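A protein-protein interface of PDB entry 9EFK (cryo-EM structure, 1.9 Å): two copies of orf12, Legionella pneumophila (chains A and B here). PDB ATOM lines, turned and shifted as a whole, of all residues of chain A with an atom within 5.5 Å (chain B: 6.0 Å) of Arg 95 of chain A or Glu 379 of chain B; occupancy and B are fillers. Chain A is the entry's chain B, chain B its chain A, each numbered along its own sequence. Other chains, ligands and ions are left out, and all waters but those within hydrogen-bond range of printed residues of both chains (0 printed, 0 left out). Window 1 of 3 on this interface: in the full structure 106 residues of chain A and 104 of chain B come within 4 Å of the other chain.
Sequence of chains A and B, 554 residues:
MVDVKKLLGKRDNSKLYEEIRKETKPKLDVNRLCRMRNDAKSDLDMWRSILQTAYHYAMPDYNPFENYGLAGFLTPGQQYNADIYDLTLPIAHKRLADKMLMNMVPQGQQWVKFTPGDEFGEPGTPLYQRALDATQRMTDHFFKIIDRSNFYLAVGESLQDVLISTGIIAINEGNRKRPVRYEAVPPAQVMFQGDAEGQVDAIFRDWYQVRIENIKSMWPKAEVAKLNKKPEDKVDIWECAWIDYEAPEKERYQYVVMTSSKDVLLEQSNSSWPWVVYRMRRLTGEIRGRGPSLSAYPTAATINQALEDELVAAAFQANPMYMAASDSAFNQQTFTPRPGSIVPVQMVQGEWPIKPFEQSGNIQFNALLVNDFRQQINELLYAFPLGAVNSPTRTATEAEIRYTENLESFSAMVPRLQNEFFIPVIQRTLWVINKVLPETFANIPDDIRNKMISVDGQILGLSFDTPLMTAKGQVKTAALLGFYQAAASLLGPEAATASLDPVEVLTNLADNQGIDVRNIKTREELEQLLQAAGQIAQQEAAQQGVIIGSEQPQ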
ATOM      1  N   PRO A  90      22.760  30.093 -28.984  1.00  0.00           N
ATOM      2  CA  PRO A  90      22.232  31.277 -28.286  1.00  0.00           C
ATOM      3  C   PRO A  90      22.820  31.491 -26.904  1.00  0.00           C
ATOM      4  O   PRO A  90      23.058  32.639 -26.515  1.00  0.00           O
ATOM      5  CB  PRO A  90      20.727  30.992 -28.226  1.00  0.00           C
ATOM      6  CG  PRO A  90      20.474  30.155 -29.404  1.00  0.00           C
ATOM      7  CD  PRO A  90      21.668  29.265 -29.525  1.00  0.00           C
ATOM      8  N   ILE A  91      23.071  30.423 -26.149  1.00  0.00           N
ATOM      9  CA  ILE A  91      23.635  30.576 -24.811  1.00  0.00           C
ATOM     10  C   ILE A  91      25.081  31.050 -24.890  1.00  0.00           C
ATOM     11  O   ILE A  91      25.476  31.999 -24.207  1.00  0.00           O
ATOM     12  CB  ILE A  91      23.513  29.261 -24.024  1.00  0.00           C
ATOM     13  CG1 ILE A  91      22.053  28.991 -23.672  1.00  0.00           C
ATOM     14  CG2 ILE A  91      24.367  29.305 -22.771  1.00  0.00           C
ATOM     15  CD1 ILE A  91      21.802  27.602 -23.157  1.00  0.00           C
ATOM     16  N   ALA A  92      25.888  30.396 -25.726  1.00  0.00           N
ATOM     17  CA  ALA A  92      27.293  30.771 -25.847  1.00  0.00           C
ATOM     18  C   ALA A  92      27.443  32.174 -26.414  1.00  0.00           C
ATOM     19  O   ALA A  92      28.325  32.929 -25.996  1.00  0.00           O
ATOM     20  CB  ALA A  92      28.030  29.760 -26.720  1.00  0.00           C
ATOM     21  N   HIS A  93      26.592  32.533 -27.375  1.00  0.00           N
ATOM     22  CA  HIS A  93      26.633  33.865 -27.965  1.00  0.00           C
ATOM     23  C   HIS A  93      26.349  34.938 -26.923  1.00  0.00           C
ATOM     24  O   HIS A  93      27.064  35.941 -26.837  1.00  0.00           O
ATOM     25  CB  HIS A  93      25.628  33.941 -29.113  1.00  0.00           C
ATOM     26  CG  HIS A  93      25.392  35.324 -29.630  1.00  0.00           C
ATOM     27  ND1 HIS A  93      26.194  35.906 -30.585  1.00  0.00           N
ATOM     28  CD2 HIS A  93      24.435  36.233 -29.336  1.00  0.00           C
ATOM     29  CE1 HIS A  93      25.745  37.118 -30.853  1.00  0.00           C
ATOM     30  NE2 HIS A  93      24.680  37.342 -30.107  1.00  0.00           N
ATOM     31  N   LYS A  94      25.309  34.739 -26.115  1.00  0.00           N
ATOM     32  CA  LYS A  94      24.959  35.730 -25.106  1.00  0.00           C
ATOM     33  C   LYS A  94      26.039  35.844 -24.040  1.00  0.00           C
ATOM     34  O   LYS A  94      26.379  36.952 -23.614  1.00  0.00           O
ATOM     35  CB  LYS A  94      23.615  35.378 -24.476  1.00  0.00           C
ATOM     36  CG  LYS A  94      23.111  36.416 -23.496  1.00  0.00           C
ATOM     37  CD  LYS A  94      21.756  36.039 -22.943  1.00  0.00           C
ATOM     38  CE  LYS A  94      21.213  37.134 -22.043  1.00  0.00           C
ATOM     39  NZ  LYS A  94      22.147  37.450 -20.930  1.00  0.00           N
ATOM     40  N   ARG A  95      26.592  34.714 -23.604  1.00  0.00           N
ATOM     41  CA  ARG A  95      27.604  34.746 -22.556  1.00  0.00           C
ATOM     42  C   ARG A  95      28.907  35.365 -23.039  1.00  0.00           C
ATOM     43  O   ARG A  95      29.610  36.003 -22.252  1.00  0.00           O
ATOM     44  CB  ARG A  95      27.847  33.339 -22.022  1.00  0.00           C
ATOM     45  CG  ARG A  95      26.761  32.851 -21.091  1.00  0.00           C
ATOM     46  CD  ARG A  95      26.879  31.364 -20.849  1.00  0.00           C
ATOM     47  NE  ARG A  95      25.801  30.867 -20.005  1.00  0.00           N
ATOM     48  CZ  ARG A  95      25.960  30.440 -18.761  1.00  0.00           C
ATOM     49  NH1 ARG A  95      27.150  30.419 -18.186  1.00  0.00           N
ATOM     50  NH2 ARG A  95      24.900  30.019 -18.080  1.00  0.00           N
ATOM     51  N   LEU A  96      29.255  35.180 -24.313  1.00  0.00           N
ATOM     52  CA  LEU A  96      30.468  35.802 -24.832  1.00  0.00           C
ATOM     53  C   LEU A  96      30.310  37.312 -24.942  1.00  0.00           C
ATOM     54  O   LEU A  96      31.236  38.061 -24.618  1.00  0.00           O
ATOM     55  CB  LEU A  96      30.837  35.203 -26.187  1.00  0.00           C
ATOM     56  CG  LEU A  96      32.035  35.838 -26.897  1.00  0.00           C
ATOM     57  CD1 LEU A  96      33.277  35.782 -26.028  1.00  0.00           C
ATOM     58  CD2 LEU A  96      32.290  35.168 -28.232  1.00  0.00           C
ATOM     59  N   ALA A  97      29.150  37.778 -25.401  1.00  0.00           N
ATOM     60  CA  ALA A  97      28.919  39.215 -25.470  1.00  0.00           C
ATOM     61  C   ALA A  97      28.929  39.840 -24.083  1.00  0.00           C
ATOM     62  O   ALA A  97      29.503  40.915 -23.884  1.00  0.00           O
ATOM     63  CB  ALA A  97      27.601  39.504 -26.182  1.00  0.00           C
ATOM     64  N   ASP A  98      28.299  39.181 -23.111  1.00  0.00           N
ATOM     65  CA  ASP A  98      28.345  39.671 -21.739  1.00  0.00           C
ATOM     66  C   ASP A  98      29.774  39.688 -21.215  1.00  0.00           C
ATOM     67  O   ASP A  98      30.188  40.638 -20.545  1.00  0.00           O
ATOM     68  CB  ASP A  98      27.463  38.808 -20.838  1.00  0.00           C
ATOM     69  CG  ASP A  98      25.991  38.899 -21.190  1.00  0.00           C
ATOM     70  OD1 ASP A  98      25.630  39.690 -22.084  1.00  0.00           O
ATOM     71  OD2 ASP A  98      25.190  38.172 -20.568  1.00  0.00           O
ATOM     72  N   LYS A  99      30.543  38.643 -21.516  1.00  0.00           N
ATOM     73  CA  LYS A  99      31.920  38.565 -21.043  1.00  0.00           C
ATOM     74  C   LYS A  99      32.776  39.668 -21.650  1.00  0.00           C
ATOM     75  O   LYS A  99      33.636  40.238 -20.971  1.00  0.00           O
ATOM     76  CB  LYS A  99      32.499  37.189 -21.364  1.00  0.00           C
ATOM     77  CG  LYS A  99      33.808  36.880 -20.686  1.00  0.00           C
ATOM     78  CD  LYS A  99      34.223  35.445 -20.954  1.00  0.00           C
ATOM     79  CE  LYS A  99      35.583  35.139 -20.354  1.00  0.00           C
ATOM     80  NZ  LYS A  99      35.609  35.336 -18.880  1.00  0.00           N
ATOM     81  N   MET A 100      32.563  39.977 -22.930  1.00  0.00           N
ATOM     82  CA  MET A 100      33.305  41.062 -23.561  1.00  0.00           C
ATOM     83  C   MET A 100      32.961  42.403 -22.931  1.00  0.00           C
ATOM     84  O   MET A 100      33.825  43.275 -22.798  1.00  0.00           O
ATOM     85  CB  MET A 100      33.024  41.094 -25.062  1.00  0.00           C
ATOM     86  CG  MET A 100      33.552  39.898 -25.825  1.00  0.00           C
ATOM     87  SD  MET A 100      33.014  39.887 -27.540  1.00  0.00           S
ATOM     88  CE  MET A 100      33.832  41.347 -28.160  1.00  0.00           C
ATOM     89  N   PHE A 384      32.088  27.362 -21.855  1.00  0.00           N
ATOM     90  CA  PHE A 384      32.036  26.053 -21.212  1.00  0.00           C
ATOM     91  C   PHE A 384      33.294  25.237 -21.481  1.00  0.00           C
ATOM     92  O   PHE A 384      33.248  24.258 -22.236  1.00  0.00           O
ATOM     93  CB  PHE A 384      30.799  25.285 -21.675  1.00  0.00           C
ATOM     94  CG  PHE A 384      29.515  26.027 -21.454  1.00  0.00           C
ATOM     95  CD1 PHE A 384      29.013  26.204 -20.178  1.00  0.00           C
ATOM     96  CD2 PHE A 384      28.814  26.555 -22.522  1.00  0.00           C
ATOM     97  CE1 PHE A 384      27.835  26.891 -19.973  1.00  0.00           C
ATOM     98  CE2 PHE A 384      27.637  27.242 -22.322  1.00  0.00           C
ATOM     99  CZ  PHE A 384      27.147  27.409 -21.047  1.00  0.00           C
ATOM    100  N   ALA A 388      29.347  20.245 -20.801  1.00  0.00           N
ATOM    101  CA  ALA A 388      28.056  20.353 -20.140  1.00  0.00           C
ATOM    102  C   ALA A 388      28.134  19.805 -18.716  1.00  0.00           C
ATOM    103  O   ALA A 388      29.187  19.372 -18.240  1.00  0.00           O
ATOM    104  CB  ALA A 388      26.983  19.631 -20.950  1.00  0.00           C
ATOM    105  N   VAL A 389      26.992  19.832 -18.024  1.00  0.00           N
ATOM    106  CA  VAL A 389      26.933  19.359 -16.643  1.00  0.00           C
ATOM    107  C   VAL A 389      27.219  17.864 -16.571  1.00  0.00           C
ATOM    108  O   VAL A 389      27.978  17.403 -15.709  1.00  0.00           O
ATOM    109  CB  VAL A 389      25.567  19.707 -16.024  1.00  0.00           C
ATOM    110  CG1 VAL A 389      25.350  18.933 -14.740  1.00  0.00           C
ATOM    111  CG2 VAL A 389      25.480  21.197 -15.764  1.00  0.00           C
ATOM    112  N   ARG B 374      16.169  19.798 -20.046  1.00  0.00           N
ATOM    113  CA  ARG B 374      16.118  20.442 -18.740  1.00  0.00           C
ATOM    114  C   ARG B 374      17.375  21.258 -18.480  1.00  0.00           C
ATOM    115  O   ARG B 374      17.305  22.362 -17.932  1.00  0.00           O
ATOM    116  CB  ARG B 374      15.932  19.402 -17.640  1.00  0.00           C
ATOM    117  CG  ARG B 374      14.521  18.901 -17.469  1.00  0.00           C
ATOM    118  CD  ARG B 374      14.469  17.873 -16.367  1.00  0.00           C
ATOM    119  NE  ARG B 374      13.115  17.411 -16.101  1.00  0.00           N
ATOM    120  CZ  ARG B 374      12.819  16.382 -15.321  1.00  0.00           C
ATOM    121  NH1 ARG B 374      13.764  15.669 -14.732  1.00  0.00           N
ATOM    122  NH2 ARG B 374      11.546  16.058 -15.129  1.00  0.00           N
ATOM    123  N   GLN B 375      18.536  20.728 -18.865  1.00  0.00           N
ATOM    124  CA  GLN B 375      19.778  21.442 -18.612  1.00  0.00           C
ATOM    125  C   GLN B 375      19.899  22.690 -19.473  1.00  0.00           C
ATOM    126  O   GLN B 375      20.507  23.674 -19.045  1.00  0.00           O
ATOM    127  CB  GLN B 375      20.973  20.519 -18.833  1.00  0.00           C
ATOM    128  CG  GLN B 375      22.291  21.119 -18.388  1.00  0.00           C
ATOM    129  CD  GLN B 375      22.220  21.734 -16.996  1.00  0.00           C
ATOM    130  OE1 GLN B 375      22.679  22.854 -16.777  1.00  0.00           O
ATOM    131  NE2 GLN B 375      21.651  20.998 -16.049  1.00  0.00           N
ATOM    132  N   GLN B 376      19.335  22.673 -20.680  1.00  0.00           N
ATOM    133  CA  GLN B 376      19.342  23.877 -21.503  1.00  0.00           C
ATOM    134  C   GLN B 376      18.549  24.995 -20.843  1.00  0.00           C
ATOM    135  O   GLN B 376      18.974  26.154 -20.848  1.00  0.00           O
ATOM    136  CB  GLN B 376      18.787  23.571 -22.891  1.00  0.00           C
ATOM    137  CG  GLN B 376      19.736  22.784 -23.760  1.00  0.00           C
ATOM    138  CD  GLN B 376      19.278  22.705 -25.195  1.00  0.00           C
ATOM    139  OE1 GLN B 376      18.109  22.926 -25.500  1.00  0.00           O
ATOM    140  NE2 GLN B 376      20.203  22.393 -26.090  1.00  0.00           N
ATOM    141  N   ILE B 377      17.396  24.664 -20.265  1.00  0.00           N
ATOM    142  CA  ILE B 377      16.620  25.655 -19.528  1.00  0.00           C
ATOM    143  C   ILE B 377      17.412  26.172 -18.337  1.00  0.00           C
ATOM    144  O   ILE B 377      17.426  27.375 -18.056  1.00  0.00           O
ATOM    145  CB  ILE B 377      15.271  25.054 -19.095  1.00  0.00           C
ATOM    146  CG1 ILE B 377      14.390  24.800 -20.314  1.00  0.00           C
ATOM    147  CG2 ILE B 377      14.574  25.961 -18.104  1.00  0.00           C
ATOM    148  CD1 ILE B 377      13.082  24.144 -19.988  1.00  0.00           C
ATOM    149  N   ASN B 378      18.082  25.272 -17.617  1.00  0.00           N
ATOM    150  CA  ASN B 378      18.844  25.677 -16.442  1.00  0.00           C
ATOM    151  C   ASN B 378      19.993  26.605 -16.813  1.00  0.00           C
ATOM    152  O   ASN B 378      20.241  27.597 -16.123  1.00  0.00           O
ATOM    153  CB  ASN B 378      19.356  24.445 -15.700  1.00  0.00           C
ATOM    154  CG  ASN B 378      18.277  23.771 -14.887  1.00  0.00           C
ATOM    155  OD1 ASN B 378      17.358  24.421 -14.403  1.00  0.00           O
ATOM    156  ND2 ASN B 378      18.384  22.461 -14.729  1.00  0.00           N
ATOM    157  N   GLU B 379      20.705  26.304 -17.900  1.00  0.00           N
ATOM    158  CA  GLU B 379      21.793  27.176 -18.331  1.00  0.00           C
ATOM    159  C   GLU B 379      21.273  28.504 -18.859  1.00  0.00           C
ATOM    160  O   GLU B 379      21.931  29.535 -18.697  1.00  0.00           O
ATOM    161  CB  GLU B 379      22.633  26.485 -19.400  1.00  0.00           C
ATOM    162  CG  GLU B 379      23.347  25.250 -18.913  1.00  0.00           C
ATOM    163  CD  GLU B 379      24.063  24.516 -20.026  1.00  0.00           C
ATOM    164  OE1 GLU B 379      24.121  25.052 -21.151  1.00  0.00           O
ATOM    165  OE2 GLU B 379      24.566  23.401 -19.775  1.00  0.00           O
ATOM    166  N   LEU B 380      20.104  28.494 -19.497  1.00  0.00           N
ATOM    167  CA  LEU B 380      19.522  29.724 -20.013  1.00  0.00           C
ATOM    168  C   LEU B 380      19.131  30.679 -18.895  1.00  0.00           C
ATOM    169  O   LEU B 380      19.140  31.897 -19.091  1.00  0.00           O
ATOM    170  CB  LEU B 380      18.308  29.386 -20.872  1.00  0.00           C
ATOM    171  CG  LEU B 380      17.631  30.485 -21.681  1.00  0.00           C
ATOM    172  CD1 LEU B 380      18.562  30.992 -22.757  1.00  0.00           C
ATOM    173  CD2 LEU B 380      16.362  29.943 -22.292  1.00  0.00           C
ATOM    174  N   LEU B 381      18.786  30.151 -17.722  1.00  0.00           N
ATOM    175  CA  LEU B 381      18.325  30.957 -16.601  1.00  0.00           C
ATOM    176  C   LEU B 381      19.314  30.972 -15.440  1.00  0.00           C
ATOM    177  O   LEU B 381      18.932  31.314 -14.319  1.00  0.00           O
ATOM    178  CB  LEU B 381      16.962  30.463 -16.125  1.00  0.00           C
ATOM    179  CG  LEU B 381      15.788  30.681 -17.075  1.00  0.00           C
ATOM    180  CD1 LEU B 381      14.505  30.334 -16.378  1.00  0.00           C
ATOM    181  CD2 LEU B 381      15.752  32.112 -17.531  1.00  0.00           C
ATOM    182  N   TYR B 382      20.571  30.602 -15.686  1.00  0.00           N
ATOM    183  CA  TYR B 382      21.635  30.668 -14.679  1.00  0.00           C
ATOM    184  C   TYR B 382      21.271  29.897 -13.413  1.00  0.00           C
ATOM    185  O   TYR B 382      21.479  30.373 -12.297  1.00  0.00           O
ATOM    186  CB  TYR B 382      21.982  32.117 -14.339  1.00  0.00           C
ATOM    187  CG  TYR B 382      22.203  32.986 -15.546  1.00  0.00           C
ATOM    188  CD1 TYR B 382      23.436  33.037 -16.170  1.00  0.00           C
ATOM    189  CD2 TYR B 382      21.177  33.761 -16.061  1.00  0.00           C
ATOM    190  CE1 TYR B 382      23.641  33.830 -17.275  1.00  0.00           C
ATOM    191  CE2 TYR B 382      21.371  34.554 -17.164  1.00  0.00           C
ATOM    192  CZ  TYR B 382      22.605  34.586 -17.768  1.00  0.00           C
ATOM    193  OH  TYR B 382      22.802  35.380 -18.870  1.00  0.00           O
ATOM    194  N   ALA B 383      20.728  28.698 -13.584  1.00  0.00           N
ATOM    195  CA  ALA B 383      20.226  27.901 -12.477  1.00  0.00           C
ATOM    196  C   ALA B 383      20.897  26.537 -12.454  1.00  0.00           C
ATOM    197  O   ALA B 383      21.232  25.975 -13.501  1.00  0.00           O
ATOM    198  CB  ALA B 383      18.709  27.724 -12.570  1.00  0.00           C
ATOM    199  N   GLU B 405      31.723  29.673 -13.326  1.00  0.00           N
ATOM    200  CA  GLU B 405      31.280  30.020 -14.671  1.00  0.00           C
ATOM    201  C   GLU B 405      29.843  30.517 -14.658  1.00  0.00           C
ATOM    202  O   GLU B 405      29.512  31.507 -15.319  1.00  0.00           O
ATOM    203  CB  GLU B 405      31.425  28.815 -15.599  1.00  0.00           C
ATOM    204  CG  GLU B 405      32.311  29.060 -16.808  1.00  0.00           C
ATOM    205  CD  GLU B 405      33.771  29.251 -16.440  1.00  0.00           C
ATOM    206  OE1 GLU B 405      34.185  28.764 -15.368  1.00  0.00           O
ATOM    207  OE2 GLU B 405      34.505  29.888 -17.223  1.00  0.00           O
ATOM    208  N   ASN B 406      28.974  29.839 -13.907  1.00  0.00           N
ATOM    209  CA  ASN B 406      27.588  30.273 -13.795  1.00  0.00           C
ATOM    210  C   ASN B 406      27.483  31.615 -13.083  1.00  0.00           C
ATOM    211  O   ASN B 406      26.695  32.476 -13.484  1.00  0.00           O
ATOM    212  CB  ASN B 406      26.774  29.205 -13.068  1.00  0.00           C
ATOM    213  CG  ASN B 406      25.298  29.516 -13.037  1.00  0.00           C
ATOM    214  OD1 ASN B 406      24.590  29.315 -14.021  1.00  0.00           O
ATOM    215  ND2 ASN B 406      24.819  29.997 -11.899  1.00  0.00           N
ATOM    216  N   SER B 409      28.776  34.607 -15.384  1.00  0.00           N
ATOM    217  CA  SER B 409      27.851  34.968 -16.454  1.00  0.00           C
ATOM    218  C   SER B 409      26.631  35.700 -15.911  1.00  0.00           C
ATOM    219  O   SER B 409      26.150  36.654 -16.530  1.00  0.00           O
ATOM    220  CB  SER B 409      27.432  33.725 -17.234  1.00  0.00           C
ATOM    221  OG  SER B 409      26.761  32.803 -16.400  1.00  0.00           O
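No position is printed for both chains.
The backbone carbonyl oxygen (O) of Tyr 382 of chain B sits at hydrogen-bond distance from the side-chain amide nitrogen (ND2) of Asn 406 of chain B (3.4 Å).
The backbone carbonyl oxygen (O) of Glu 405 of chain B sits at hydrogen-bond distance from the side-chain hydroxyl (OG) of Ser 409 of chain B (3.2 Å).
O of Asn 406 of chain B lies within hydrogen-bond range of OG of Ser 409 of chain B, 2.9 Å away.
The side-chain carboxylate of Asp 98 of chain A lies within salt-bridge range of the side-chain amino group of Lys 94 of chain A, at 3.1 Å.
The backbone carbonyl oxygen (O) of Glu 379 of chain B sits at hydrogen-bond distance from the guanidinium group (NH2) of Arg 95 of chain A (3.1 Å).
OH of Tyr 382 of chain B is in hydrogen-bond range of NZ of Lys 94 of chain A, 3.0 Å away.
The guanidinium group (NH1) of Arg 95 of chain A lies within hydrogen-bond range of the side-chain hydroxyl (OG) of Ser 409 of chain B.
Of the printed residues of chain B, Ile 91 of chain A touches Gln 376 (3.9 Å) and Glu 379 (3.99 Å).
Arg 95 of chain A touches four residues of chain B.
Met 100 of chain A touches none of the printed residues of chain B.
Printed residues of chain B within 4 Å of Phe 384 of chain A: Glu 379.
Ala 388 of chain A touches none of the printed residues of chain B.
Printed residues of chain A within 4 Å of Gln 376 of chain B: Ile 91 (3.9 Å).
Of the printed residues of chain A, Tyr 382 of chain B touches Lys 94 (3.0 Å) and Arg 95 (3.9 Å).
Printed residues of chain A within 4 Å of Glu 405 of chain B: Arg 95 (3.9 Å).
The nearest printed residue of chain A that does not touch Glu 379 of chain B is Ala 388 of chain A (4.6 Å).
The nearest printed residue of chain B that does not touch Val 389 of chain A is Glu 379 of chain B (4.7 Å).
Hydrophobic or aromatic side chains of chain B that line the printed part of chain A: Tyr 382.
Of the 14 printed residues of chain A, 5 touch a printed residue of chain B.
Among the printed residues, no Asp or Glu carboxylate lies within 4 Å of a Lys or Arg side-chain nitrogen of the other chain.
Among the printed residues, pairs that only touch across the chains: Val 389 of chain A with Gln 375 of chain B, Phe 384 of chain A with Glu 379 of chain B, Arg 95 of chain A with Tyr 382 of chain B, Arg 95 of chain A with Glu 405 of chain B, Ile 91 of chain A with Gln 376 of chain B and Ile 91 of chain A with Glu 379 of chain B.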
